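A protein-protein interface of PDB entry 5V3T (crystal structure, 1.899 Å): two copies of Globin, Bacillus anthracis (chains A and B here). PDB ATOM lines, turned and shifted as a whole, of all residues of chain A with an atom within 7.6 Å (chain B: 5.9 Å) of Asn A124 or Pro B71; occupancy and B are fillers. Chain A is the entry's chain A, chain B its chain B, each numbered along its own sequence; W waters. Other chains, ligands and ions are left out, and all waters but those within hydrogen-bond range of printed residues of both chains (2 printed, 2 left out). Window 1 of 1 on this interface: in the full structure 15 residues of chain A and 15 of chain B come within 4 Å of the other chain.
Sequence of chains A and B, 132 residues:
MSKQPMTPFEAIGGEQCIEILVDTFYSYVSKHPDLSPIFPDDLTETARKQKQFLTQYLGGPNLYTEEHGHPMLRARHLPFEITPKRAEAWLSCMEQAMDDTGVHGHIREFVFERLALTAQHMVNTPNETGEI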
ATOM      1  N   LEU A  73     -11.090  18.408   1.668  1.00  0.00           N
ATOM      2  CA  LEU A  73      -9.653  18.632   1.655  1.00  0.00           C
ATOM      3  C   LEU A  73      -8.967  18.067   2.872  1.00  0.00           C
ATOM      4  O   LEU A  73      -7.875  17.515   2.747  1.00  0.00           O
ATOM      5  CB  LEU A  73      -9.335  20.116   1.531  1.00  0.00           C
ATOM      6  CG  LEU A  73      -9.407  20.664   0.102  1.00  0.00           C
ATOM      7  CD1 LEU A  73      -8.660  21.978   0.039  1.00  0.00           C
ATOM      8  CD2 LEU A  73      -8.845  19.657  -0.910  1.00  0.00           C
ATOM      9  N   ARG A  74      -9.570  18.216   4.050  1.00  0.00           N
ATOM     10  CA  ARG A  74      -8.914  17.689   5.253  1.00  0.00           C
ATOM     11  C   ARG A  74      -8.694  16.202   5.119  1.00  0.00           C
ATOM     12  O   ARG A  74      -7.640  15.685   5.497  1.00  0.00           O
ATOM     13  CB  ARG A  74      -9.727  17.957   6.518  1.00  0.00           C
ATOM     14  CG  ARG A  74      -9.080  17.277   7.732  1.00  0.00           C
ATOM     15  CD  ARG A  74      -9.786  17.519   9.053  1.00  0.00           C
ATOM     16  NE  ARG A  74      -9.140  16.775  10.138  1.00  0.00           N
ATOM     17  CZ  ARG A  74      -7.950  17.057  10.671  1.00  0.00           C
ATOM     18  NH1 ARG A  74      -7.465  16.293  11.649  1.00  0.00           N
ATOM     19  NH2 ARG A  74      -7.240  18.093  10.236  1.00  0.00           N
ATOM     20  N   ALA A  75      -9.695  15.515   4.581  1.00  0.00           N
ATOM     21  CA  ALA A  75      -9.593  14.080   4.417  1.00  0.00           C
ATOM     22  C   ALA A  75      -8.483  13.752   3.418  1.00  0.00           C
ATOM     23  O   ALA A  75      -7.686  12.849   3.646  1.00  0.00           O
ATOM     24  CB  ALA A  75     -10.953  13.482   3.957  1.00  0.00           C
ATOM     25  N   ARG A  76      -8.402  14.529   2.335  1.00  0.00           N
ATOM     26  CA  ARG A  76      -7.387  14.278   1.306  1.00  0.00           C
ATOM     27  C   ARG A  76      -5.954  14.562   1.773  1.00  0.00           C
ATOM     28  O   ARG A  76      -4.997  14.042   1.200  1.00  0.00           O
ATOM     29  CB  ARG A  76      -7.674  15.097   0.061  1.00  0.00           C
ATOM     30  CG  ARG A  76      -8.962  14.712  -0.661  1.00  0.00           C
ATOM     31  CD  ARG A  76      -9.034  15.448  -1.994  1.00  0.00           C
ATOM     32  NE  ARG A  76     -10.314  15.254  -2.688  1.00  0.00           N
ATOM     33  CZ  ARG A  76     -10.500  14.376  -3.671  1.00  0.00           C
ATOM     34  NH1 ARG A  76     -11.686  14.267  -4.255  1.00  0.00           N
ATOM     35  NH2 ARG A  76      -9.491  13.617  -4.083  1.00  0.00           N
ATOM     36  N   HIS A  77      -5.815  15.368   2.817  1.00  0.00           N
ATOM     37  CA  HIS A  77      -4.496  15.709   3.372  1.00  0.00           C
ATOM     38  C   HIS A  77      -4.066  14.858   4.564  1.00  0.00           C
ATOM     39  O   HIS A  77      -2.968  15.046   5.095  1.00  0.00           O
ATOM     40  CB  HIS A  77      -4.469  17.174   3.779  1.00  0.00           C
ATOM     41  CG  HIS A  77      -4.363  18.113   2.625  1.00  0.00           C
ATOM     42  ND1 HIS A  77      -5.449  18.474   1.858  1.00  0.00           N
ATOM     43  CD2 HIS A  77      -3.299  18.773   2.108  1.00  0.00           C
ATOM     44  CE1 HIS A  77      -5.061  19.325   0.925  1.00  0.00           C
ATOM     45  NE2 HIS A  77      -3.761  19.521   1.051  1.00  0.00           N
ATOM     46  N   LEU A  78      -4.935  13.946   4.990  1.00  0.00           N
ATOM     47  CA  LEU A  78      -4.669  13.098   6.148  1.00  0.00           C
ATOM     48  C   LEU A  78      -3.321  12.346   6.118  1.00  0.00           C
ATOM     49  O   LEU A  78      -2.668  12.249   7.169  1.00  0.00           O
ATOM     50  CB  LEU A  78      -5.793  12.059   6.313  1.00  0.00           C
ATOM     51  CG  LEU A  78      -7.176  12.474   6.828  1.00  0.00           C
ATOM     52  CD1 LEU A  78      -8.055  11.243   6.986  1.00  0.00           C
ATOM     53  CD2 LEU A  78      -7.121  13.253   8.125  1.00  0.00           C
ATOM     54  N   PRO A  79      -2.900  11.800   4.951  1.00  0.00           N
ATOM     55  CA  PRO A  79      -1.657  11.020   5.030  1.00  0.00           C
ATOM     56  C   PRO A  79      -0.402  11.882   5.076  1.00  0.00           C
ATOM     57  O   PRO A  79       0.675  11.353   5.351  1.00  0.00           O
ATOM     58  CB  PRO A  79      -1.652  10.208   3.727  1.00  0.00           C
ATOM     59  CG  PRO A  79      -3.032  10.361   3.142  1.00  0.00           C
ATOM     60  CD  PRO A  79      -3.510  11.682   3.616  1.00  0.00           C
ATOM     61  N   PHE A  80      -0.541  13.184   4.855  1.00  0.00           N
ATOM     62  CA  PHE A  80       0.642  14.041   4.758  1.00  0.00           C
ATOM     63  C   PHE A  80       0.943  14.738   6.077  1.00  0.00           C
ATOM     64  O   PHE A  80       0.036  15.047   6.851  1.00  0.00           O
ATOM     65  CB  PHE A  80       0.460  15.070   3.639  1.00  0.00           C
ATOM     66  CG  PHE A  80      -0.003  14.469   2.341  1.00  0.00           C
ATOM     67  CD1 PHE A  80       0.774  13.529   1.682  1.00  0.00           C
ATOM     68  CD2 PHE A  80      -1.193  14.882   1.753  1.00  0.00           C
ATOM     69  CE1 PHE A  80       0.356  12.981   0.481  1.00  0.00           C
ATOM     70  CE2 PHE A  80      -1.613  14.342   0.551  1.00  0.00           C
ATOM     71  CZ  PHE A  80      -0.842  13.394  -0.085  1.00  0.00           C
ATOM     72  N   GLU A  81       2.226  14.948   6.352  1.00  0.00           N
ATOM     73  CA  GLU A  81       2.618  15.546   7.620  1.00  0.00           C
ATOM     74  C   GLU A  81       2.425  17.053   7.594  1.00  0.00           C
ATOM     75  O   GLU A  81       3.354  17.790   7.288  1.00  0.00           O
ATOM     76  CB  GLU A  81       4.074  15.208   7.945  1.00  0.00           C
ATOM     77  CG  GLU A  81       4.506  15.699   9.310  1.00  0.00           C
ATOM     78  CD  GLU A  81       5.873  15.179   9.710  1.00  0.00           C
ATOM     79  OE1 GLU A  81       6.820  15.342   8.911  1.00  0.00           O
ATOM     80  OE2 GLU A  81       5.989  14.602  10.810  1.00  0.00           O
ATOM     81  N   ILE A  82       1.220  17.508   7.923  1.00  0.00           N
ATOM     82  CA  ILE A  82       0.933  18.937   7.899  1.00  0.00           C
ATOM     83  C   ILE A  82       0.976  19.497   9.321  1.00  0.00           C
ATOM     84  O   ILE A  82       0.023  19.398  10.098  1.00  0.00           O
ATOM     85  CB  ILE A  82      -0.413  19.227   7.235  1.00  0.00           C
ATOM     86  CG1 ILE A  82      -0.437  18.575   5.852  1.00  0.00           C
ATOM     87  CG2 ILE A  82      -0.654  20.743   7.121  1.00  0.00           C
ATOM     88  CD1 ILE A  82      -1.683  18.845   5.098  1.00  0.00           C
ATOM     89  N   THR A  83       2.117  20.096   9.641  1.00  0.00           N
ATOM     90  CA  THR A  83       2.363  20.700  10.928  1.00  0.00           C
ATOM     91  C   THR A  83       1.896  22.143  10.880  1.00  0.00           C
ATOM     92  O   THR A  83       1.710  22.696   9.791  1.00  0.00           O
ATOM     93  CB  THR A  83       3.846  20.670  11.252  1.00  0.00           C
ATOM     94  OG1 THR A  83       4.542  21.295  10.166  1.00  0.00           O
ATOM     95  CG2 THR A  83       4.320  19.237  11.393  1.00  0.00           C
ATOM     96  N   PRO A  84       1.700  22.767  12.053  1.00  0.00           N
ATOM     97  CA  PRO A  84       1.415  24.207  12.017  1.00  0.00           C
ATOM     98  C   PRO A  84       2.528  24.985  11.304  1.00  0.00           C
ATOM     99  O   PRO A  84       2.243  25.979  10.630  1.00  0.00           O
ATOM    100  CB  PRO A  84       1.324  24.580  13.495  1.00  0.00           C
ATOM    101  CG  PRO A  84       0.893  23.304  14.171  1.00  0.00           C
ATOM    102  CD  PRO A  84       1.590  22.212  13.416  1.00  0.00           C
ATOM    103  N   ALA A 119      -6.167  26.289   5.497  1.00  0.00           N
ATOM    104  CA  ALA A 119      -4.848  25.741   5.826  1.00  0.00           C
ATOM    105  C   ALA A 119      -4.775  25.276   7.277  1.00  0.00           C
ATOM    106  O   ALA A 119      -4.128  24.265   7.584  1.00  0.00           O
ATOM    107  CB  ALA A 119      -3.771  26.777   5.546  1.00  0.00           C
ATOM    108  N   GLN A 120      -5.427  26.016   8.174  1.00  0.00           N
ATOM    109  CA  GLN A 120      -5.521  25.596   9.571  1.00  0.00           C
ATOM    110  C   GLN A 120      -6.281  24.288   9.711  1.00  0.00           C
ATOM    111  O   GLN A 120      -5.942  23.448  10.553  1.00  0.00           O
ATOM    112  CB  GLN A 120      -6.192  26.660  10.435  1.00  0.00           C
ATOM    113  CG  GLN A 120      -6.303  26.250  11.909  1.00  0.00           C
ATOM    114  CD  GLN A 120      -4.949  25.945  12.553  1.00  0.00           C
ATOM    115  OE1 GLN A 120      -3.979  26.681  12.369  1.00  0.00           O
ATOM    116  NE2 GLN A 120      -4.883  24.848  13.306  1.00  0.00           N
ATOM    117  N   HIS A 121      -7.313  24.121   8.891  1.00  0.00           N
ATOM    118  CA  HIS A 121      -8.121  22.906   8.919  1.00  0.00           C
ATOM    119  C   HIS A 121      -7.336  21.674   8.477  1.00  0.00           C
ATOM    120  O   HIS A 121      -7.640  20.556   8.902  1.00  0.00           O
ATOM    121  CB  HIS A 121      -9.361  23.072   8.028  1.00  0.00           C
ATOM    122  CG  HIS A 121     -10.454  22.088   8.321  1.00  0.00           C
ATOM    123  ND1 HIS A 121     -11.204  21.489   7.331  1.00  0.00           N
ATOM    124  CD2 HIS A 121     -10.933  21.612   9.495  1.00  0.00           C
ATOM    125  CE1 HIS A 121     -12.091  20.678   7.881  1.00  0.00           C
ATOM    126  NE2 HIS A 121     -11.949  20.737   9.193  1.00  0.00           N
ATOM    127  N   MET A 122      -6.346  21.888   7.611  1.00  0.00           N
ATOM    128  CA  MET A 122      -5.526  20.809   7.071  1.00  0.00           C
ATOM    129  C   MET A 122      -4.531  20.245   8.105  1.00  0.00           C
ATOM    130  O   MET A 122      -4.152  19.084   8.012  1.00  0.00           O
ATOM    131  CB  MET A 122      -4.754  21.286   5.835  1.00  0.00           C
ATOM    132  CG  MET A 122      -5.605  21.847   4.696  1.00  0.00           C
ATOM    133  SD  MET A 122      -6.801  20.638   4.120  1.00  0.00           S
ATOM    134  CE  MET A 122      -8.294  21.242   4.934  1.00  0.00           C
ATOM    135  N   VAL A 123      -4.129  21.065   9.078  1.00  0.00           N
ATOM    136  CA  VAL A 123      -3.110  20.668  10.073  1.00  0.00           C
ATOM    137  C   VAL A 123      -3.491  19.360  10.747  1.00  0.00           C
ATOM    138  O   VAL A 123      -4.612  19.209  11.222  1.00  0.00           O
ATOM    139  CB  VAL A 123      -2.905  21.748  11.157  1.00  0.00           C
ATOM    140  CG1 VAL A 123      -2.008  21.207  12.293  1.00  0.00           C
ATOM    141  CG2 VAL A 123      -2.314  23.002  10.540  1.00  0.00           C
ATOM    142  N   ASN A 124      -2.561  18.408  10.779  1.00  0.00           N
ATOM    143  CA  ASN A 124      -2.887  17.079  11.259  1.00  0.00           C
ATOM    144  C   ASN A 124      -1.779  16.450  12.120  1.00  0.00           C
ATOM    145  O   ASN A 124      -1.841  15.280  12.445  1.00  0.00           O
ATOM    146  CB  ASN A 124      -3.233  16.171  10.072  1.00  0.00           C
ATOM    147  CG  ASN A 124      -2.133  16.113   9.021  1.00  0.00           C
ATOM    148  OD1 ASN A 124      -0.934  16.134   9.331  1.00  0.00           O
ATOM    149  ND2 ASN A 124      -2.541  15.994   7.770  1.00  0.00           N
ATOM    150  N   THR A 125      -0.773  17.257  12.453  1.00  0.00           N
ATOM    151  CA  THR A 125       0.403  16.833  13.232  1.00  0.00           C
ATOM    152  C   THR A 125       0.723  17.957  14.214  1.00  0.00           C
ATOM    153  O   THR A 125       0.597  19.124  13.853  1.00  0.00           O
ATOM    154  CB  THR A 125       1.608  16.578  12.315  1.00  0.00           C
ATOM    155  OG1 THR A 125       1.214  15.709  11.244  1.00  0.00           O
ATOM    156  CG2 THR A 125       2.806  16.005  13.079  1.00  0.00           C
ATOM    157  N   PRO A 126       1.070  17.627  15.469  1.00  0.00           N
ATOM    158  CA  PRO A 126       1.376  18.740  16.385  1.00  0.00           C
ATOM    159  C   PRO A 126       2.693  19.475  16.080  1.00  0.00           C
ATOM    160  O   PRO A 126       3.523  18.990  15.310  1.00  0.00           O
ATOM    161  CB  PRO A 126       1.440  18.054  17.754  1.00  0.00           C
ATOM    162  CG  PRO A 126       1.700  16.643  17.472  1.00  0.00           C
ATOM    163  CD  PRO A 126       1.118  16.315  16.145  1.00  0.00           C
ATOM    164  N   PHE B  53      -8.888   4.199   8.813  1.00  0.00           N
ATOM    165  CA  PHE B  53      -8.081   5.223   8.165  1.00  0.00           C
ATOM    166  C   PHE B  53      -8.420   5.332   6.681  1.00  0.00           C
ATOM    167  O   PHE B  53      -8.698   6.416   6.194  1.00  0.00           O
ATOM    168  CB  PHE B  53      -6.578   4.971   8.322  1.00  0.00           C
ATOM    169  CG  PHE B  53      -5.753   6.132   7.821  1.00  0.00           C
ATOM    170  CD1 PHE B  53      -5.573   7.240   8.623  1.00  0.00           C
ATOM    171  CD2 PHE B  53      -5.292   6.172   6.518  1.00  0.00           C
ATOM    172  CE1 PHE B  53      -4.868   8.372   8.154  1.00  0.00           C
ATOM    173  CE2 PHE B  53      -4.587   7.300   6.031  1.00  0.00           C
ATOM    174  CZ  PHE B  53      -4.384   8.392   6.853  1.00  0.00           C
ATOM    175  N   TYR B  64     -11.487   7.235  11.677  1.00  0.00           N
ATOM    176  CA  TYR B  64     -10.167   7.216  12.290  1.00  0.00           C
ATOM    177  C   TYR B  64      -9.953   8.340  13.302  1.00  0.00           C
ATOM    178  O   TYR B  64      -9.646   8.074  14.471  1.00  0.00           O
ATOM    179  CB  TYR B  64      -9.055   7.254  11.226  1.00  0.00           C
ATOM    180  CG  TYR B  64      -7.699   7.084  11.856  1.00  0.00           C
ATOM    181  CD1 TYR B  64      -7.158   5.818  12.070  1.00  0.00           C
ATOM    182  CD2 TYR B  64      -6.972   8.188  12.293  1.00  0.00           C
ATOM    183  CE1 TYR B  64      -5.911   5.663  12.696  1.00  0.00           C
ATOM    184  CE2 TYR B  64      -5.744   8.042  12.906  1.00  0.00           C
ATOM    185  CZ  TYR B  64      -5.219   6.778  13.108  1.00  0.00           C
ATOM    186  OH  TYR B  64      -3.993   6.657  13.717  1.00  0.00           O
ATOM    187  N   THR B  65     -10.084   9.593  12.864  1.00  0.00           N
ATOM    188  CA  THR B  65      -9.753  10.714  13.733  1.00  0.00           C
ATOM    189  C   THR B  65     -10.696  10.792  14.942  1.00  0.00           C
ATOM    190  O   THR B  65     -10.288  11.221  16.025  1.00  0.00           O
ATOM    191  CB  THR B  65      -9.746  12.050  12.959  1.00  0.00           C
ATOM    192  OG1 THR B  65     -11.028  12.290  12.364  1.00  0.00           O
ATOM    193  CG2 THR B  65      -8.668  12.015  11.882  1.00  0.00           C
ATOM    194  N   GLY B  69      -7.742  10.606  17.239  1.00  0.00           N
ATOM    195  CA  GLY B  69      -7.198  11.959  17.191  1.00  0.00           C
ATOM    196  C   GLY B  69      -6.537  12.309  15.866  1.00  0.00           C
ATOM    197  O   GLY B  69      -6.867  11.737  14.827  1.00  0.00           O
ATOM    198  N   HIS B  70      -5.639  13.290  15.880  1.00  0.00           N
ATOM    199  CA  HIS B  70      -4.928  13.657  14.656  1.00  0.00           C
ATOM    200  C   HIS B  70      -4.178  12.451  14.105  1.00  0.00           C
ATOM    201  O   HIS B  70      -3.646  11.641  14.867  1.00  0.00           O
ATOM    202  CB  HIS B  70      -3.963  14.824  14.893  1.00  0.00           C
ATOM    203  CG  HIS B  70      -4.653  16.133  15.100  1.00  0.00           C
ATOM    204  ND1 HIS B  70      -5.453  16.706  14.137  1.00  0.00           N
ATOM    205  CD2 HIS B  70      -4.665  16.980  16.155  1.00  0.00           C
ATOM    206  CE1 HIS B  70      -5.932  17.851  14.589  1.00  0.00           C
ATOM    207  NE2 HIS B  70      -5.470  18.041  15.812  1.00  0.00           N
ATOM    208  N   PRO B  71      -4.171  12.312  12.775  1.00  0.00           N
ATOM    209  CA  PRO B  71      -3.520  11.225  12.039  1.00  0.00           C
ATOM    210  C   PRO B  71      -2.034  11.139  12.312  1.00  0.00           C
ATOM    211  O   PRO B  71      -1.536  10.048  12.621  1.00  0.00           O
ATOM    212  CB  PRO B  71      -3.742  11.610  10.574  1.00  0.00           C
ATOM    213  CG  PRO B  71      -4.875  12.506  10.598  1.00  0.00           C
ATOM    214  CD  PRO B  71      -4.835  13.258  11.865  1.00  0.00           C
ATOM    215  N   MET B  72      -1.353  12.278  12.180  1.00  0.00           N
ATOM    216  CA  MET B  72       0.112  12.379  12.342  1.00  0.00           C
ATOM    217  C   MET B  72       0.793  11.095  11.856  1.00  0.00           C
ATOM    218  O   MET B  72       1.581  10.455  12.566  1.00  0.00           O
ATOM    219  CB  MET B  72       0.484  12.704  13.804  1.00  0.00           C
ATOM    220  CG  MET B  72       0.184  11.622  14.854  1.00  0.00           C
ATOM    221  SD  MET B  72       0.582  12.219  16.489  1.00  0.00           S
ATOM    222  CE  MET B  72      -0.860  13.225  16.844  1.00  0.00           C
ATOM    223  N   LEU B  73       0.476  10.726  10.619  1.00  0.00           N
ATOM    224  CA  LEU B  73       0.751   9.386  10.139  1.00  0.00           C
ATOM    225  C   LEU B  73       2.239   9.019  10.139  1.00  0.00           C
ATOM    226  O   LEU B  73       2.621   7.946  10.617  1.00  0.00           O
ATOM    227  CB  LEU B  73       0.164   9.226   8.728  1.00  0.00           C
ATOM    228  CG  LEU B  73      -0.008   7.771   8.293  1.00  0.00           C
ATOM    229  CD1 LEU B  73      -0.989   7.034   9.217  1.00  0.00           C
ATOM    230  CD2 LEU B  73      -0.456   7.683   6.846  1.00  0.00           C
ATOM    231  N   ARG B  74       3.088   9.914   9.652  1.00  0.00           N
ATOM    232  CA  ARG B  74       4.503   9.586   9.583  1.00  0.00           C
ATOM    233  C   ARG B  74       5.038   9.365  10.993  1.00  0.00           C
ATOM    234  O   ARG B  74       5.845   8.469  11.214  1.00  0.00           O
ATOM    235  CB  ARG B  74       5.315  10.678   8.881  1.00  0.00           C
ATOM    236  CG  ARG B  74       6.783  10.262   8.660  1.00  0.00           C
ATOM    237  CD  ARG B  74       7.587  11.280   7.893  1.00  0.00           C
ATOM    238  NE  ARG B  74       8.913  10.747   7.554  1.00  0.00           N
ATOM    239  CZ  ARG B  74      10.025  10.953   8.254  1.00  0.00           C
ATOM    240  NH1 ARG B  74      10.009  11.699   9.353  1.00  0.00           N
ATOM    241  NH2 ARG B  74      11.157  10.404   7.845  1.00  0.00           N
ATOM    242  N   ARG B  76       3.570   8.263  13.597  1.00  0.00           N
ATOM    243  CA  ARG B  76       3.128   6.979  14.091  1.00  0.00           C
ATOM    244  C   ARG B  76       3.986   5.859  13.513  1.00  0.00           C
ATOM    245  O   ARG B  76       4.018   4.748  14.054  1.00  0.00           O
ATOM    246  CB  ARG B  76       1.648   6.750  13.740  1.00  0.00           C
ATOM    247  CG  ARG B  76       0.716   7.735  14.417  1.00  0.00           C
ATOM    248  CD  ARG B  76      -0.755   7.340  14.246  1.00  0.00           C
ATOM    249  NE  ARG B  76      -1.679   8.385  14.695  1.00  0.00           N
ATOM    250  CZ  ARG B  76      -2.236   8.432  15.903  1.00  0.00           C
ATOM    251  NH1 ARG B  76      -1.924   7.518  16.821  1.00  0.00           N
ATOM    252  NH2 ARG B  76      -3.076   9.416  16.210  1.00  0.00           N
HETATM  253  O   HOH W   1       8.124  13.279  10.907  1.00  0.00           O
HETATM  254  O   HOH W   2       3.189  12.848  11.123  1.00  0.00           O
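The backbone NH of Met B72 is in hydrogen-bond range of the backbone carbonyl oxygen of Asn A124 (3.1 Å). A ring nitrogen (ND1) of His B70 is in hydrogen-bond range of the guanidinium group (NH1) of Arg A74 (3.2 Å).
Water W1 bridges OE2 of Glu A81 and NH1 of Arg B74. Water W2 lies within hydrogen-bond range of the backbone carbonyl oxygen (O) of Met B72 (3.2 Å), the backbone NH (N) of Arg B74 (3.3 Å), the side-chain carboxylate (OE2) of Glu A81 (3.3 Å), the side-chain hydroxyl (OG1) of Thr A125 (3.5 Å) and the backbone NH (N) of Leu B73 (3.5 Å).
3 positions are printed for both chains. Of the 10 pairs that touch across the chains among the printed residues, none has its exchanged pair printed and touching as well.
Printed residues of chain B that touch a printed residue of chain A: Phe B53, His B70, Pro B71, Met B72 and Leu B73. Hydrophobic or aromatic side chains of chain B that line the printed part of chain A: Phe B53, His B70, Pro B71, Met B72 and Leu B73. Of the 20 printed residues of chain A, 7 touch a printed residue of chain B. Among the printed residues, 10 pairs touch across the chains.
Of the printed residues of chain B, Pro A79 touches Leu B73. Asn A124 touches three residues of chain B. Printed residues of chain B within 4 Å of Pro A126: Met B72 (3.7 Å). Printed residues of chain A within 4 Å of Phe B53: Leu A78 (3.97 Å). Of chain A, only Leu A78 and Asn A124 come within 4 Å of Pro B71. Of the printed residues of chain A, Met B72 touches Asn A124, Thr A125 and Pro A126. The nearest residue of chain B that does not touch Asn A124 is Leu B73 (5.4 Å). The nearest residue of chain A that does not touch Pro B71 is Arg A74 (4.02 Å). The nearest printed residue of chain B that does not touch Pro A79 is Phe B53 (4.2 Å).
Among the printed residues, merely in contact across the chains: Asn A124 with His B70 (3.3 Å), Leu A78 with Pro B71 (3.4 Å), Asn A124 with Pro B71 (3.7 Å), Thr A125 with Met B72 (3.7 Å), Pro A126 with Met B72 (3.7 Å), Val A123 with His B70 (3.9 Å), Leu A78 with Phe B53 (3.97 Å) and Pro A79 with Leu B73 (3.98 Å).
The side-chain sulfur (SD) of Met A122 sits close to the backbone NH (N) of Arg A74 (3.7 Å). The side-chain amide nitrogen of Asn A124 sits at hydrogen-bond distance from the backbone carbonyl oxygen of His A77 (2.9 Å). The backbone carbonyl oxygen (O) of Ile A82 sits at hydrogen-bond distance from the backbone NH (N) of Thr A125, at 3.3 Å. The backbone carbonyl oxygen (O) of His B70 sits at hydrogen-bond distance from the guanidinium group (NH2) of Arg B76. The guanidinium group (NH2) of Arg A74 lies within hydrogen-bond range of the backbone carbonyl oxygen (O) of His A121 (2.8 Å). ND2 of Asn A124 is in hydrogen-bond range of O of Met A122.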
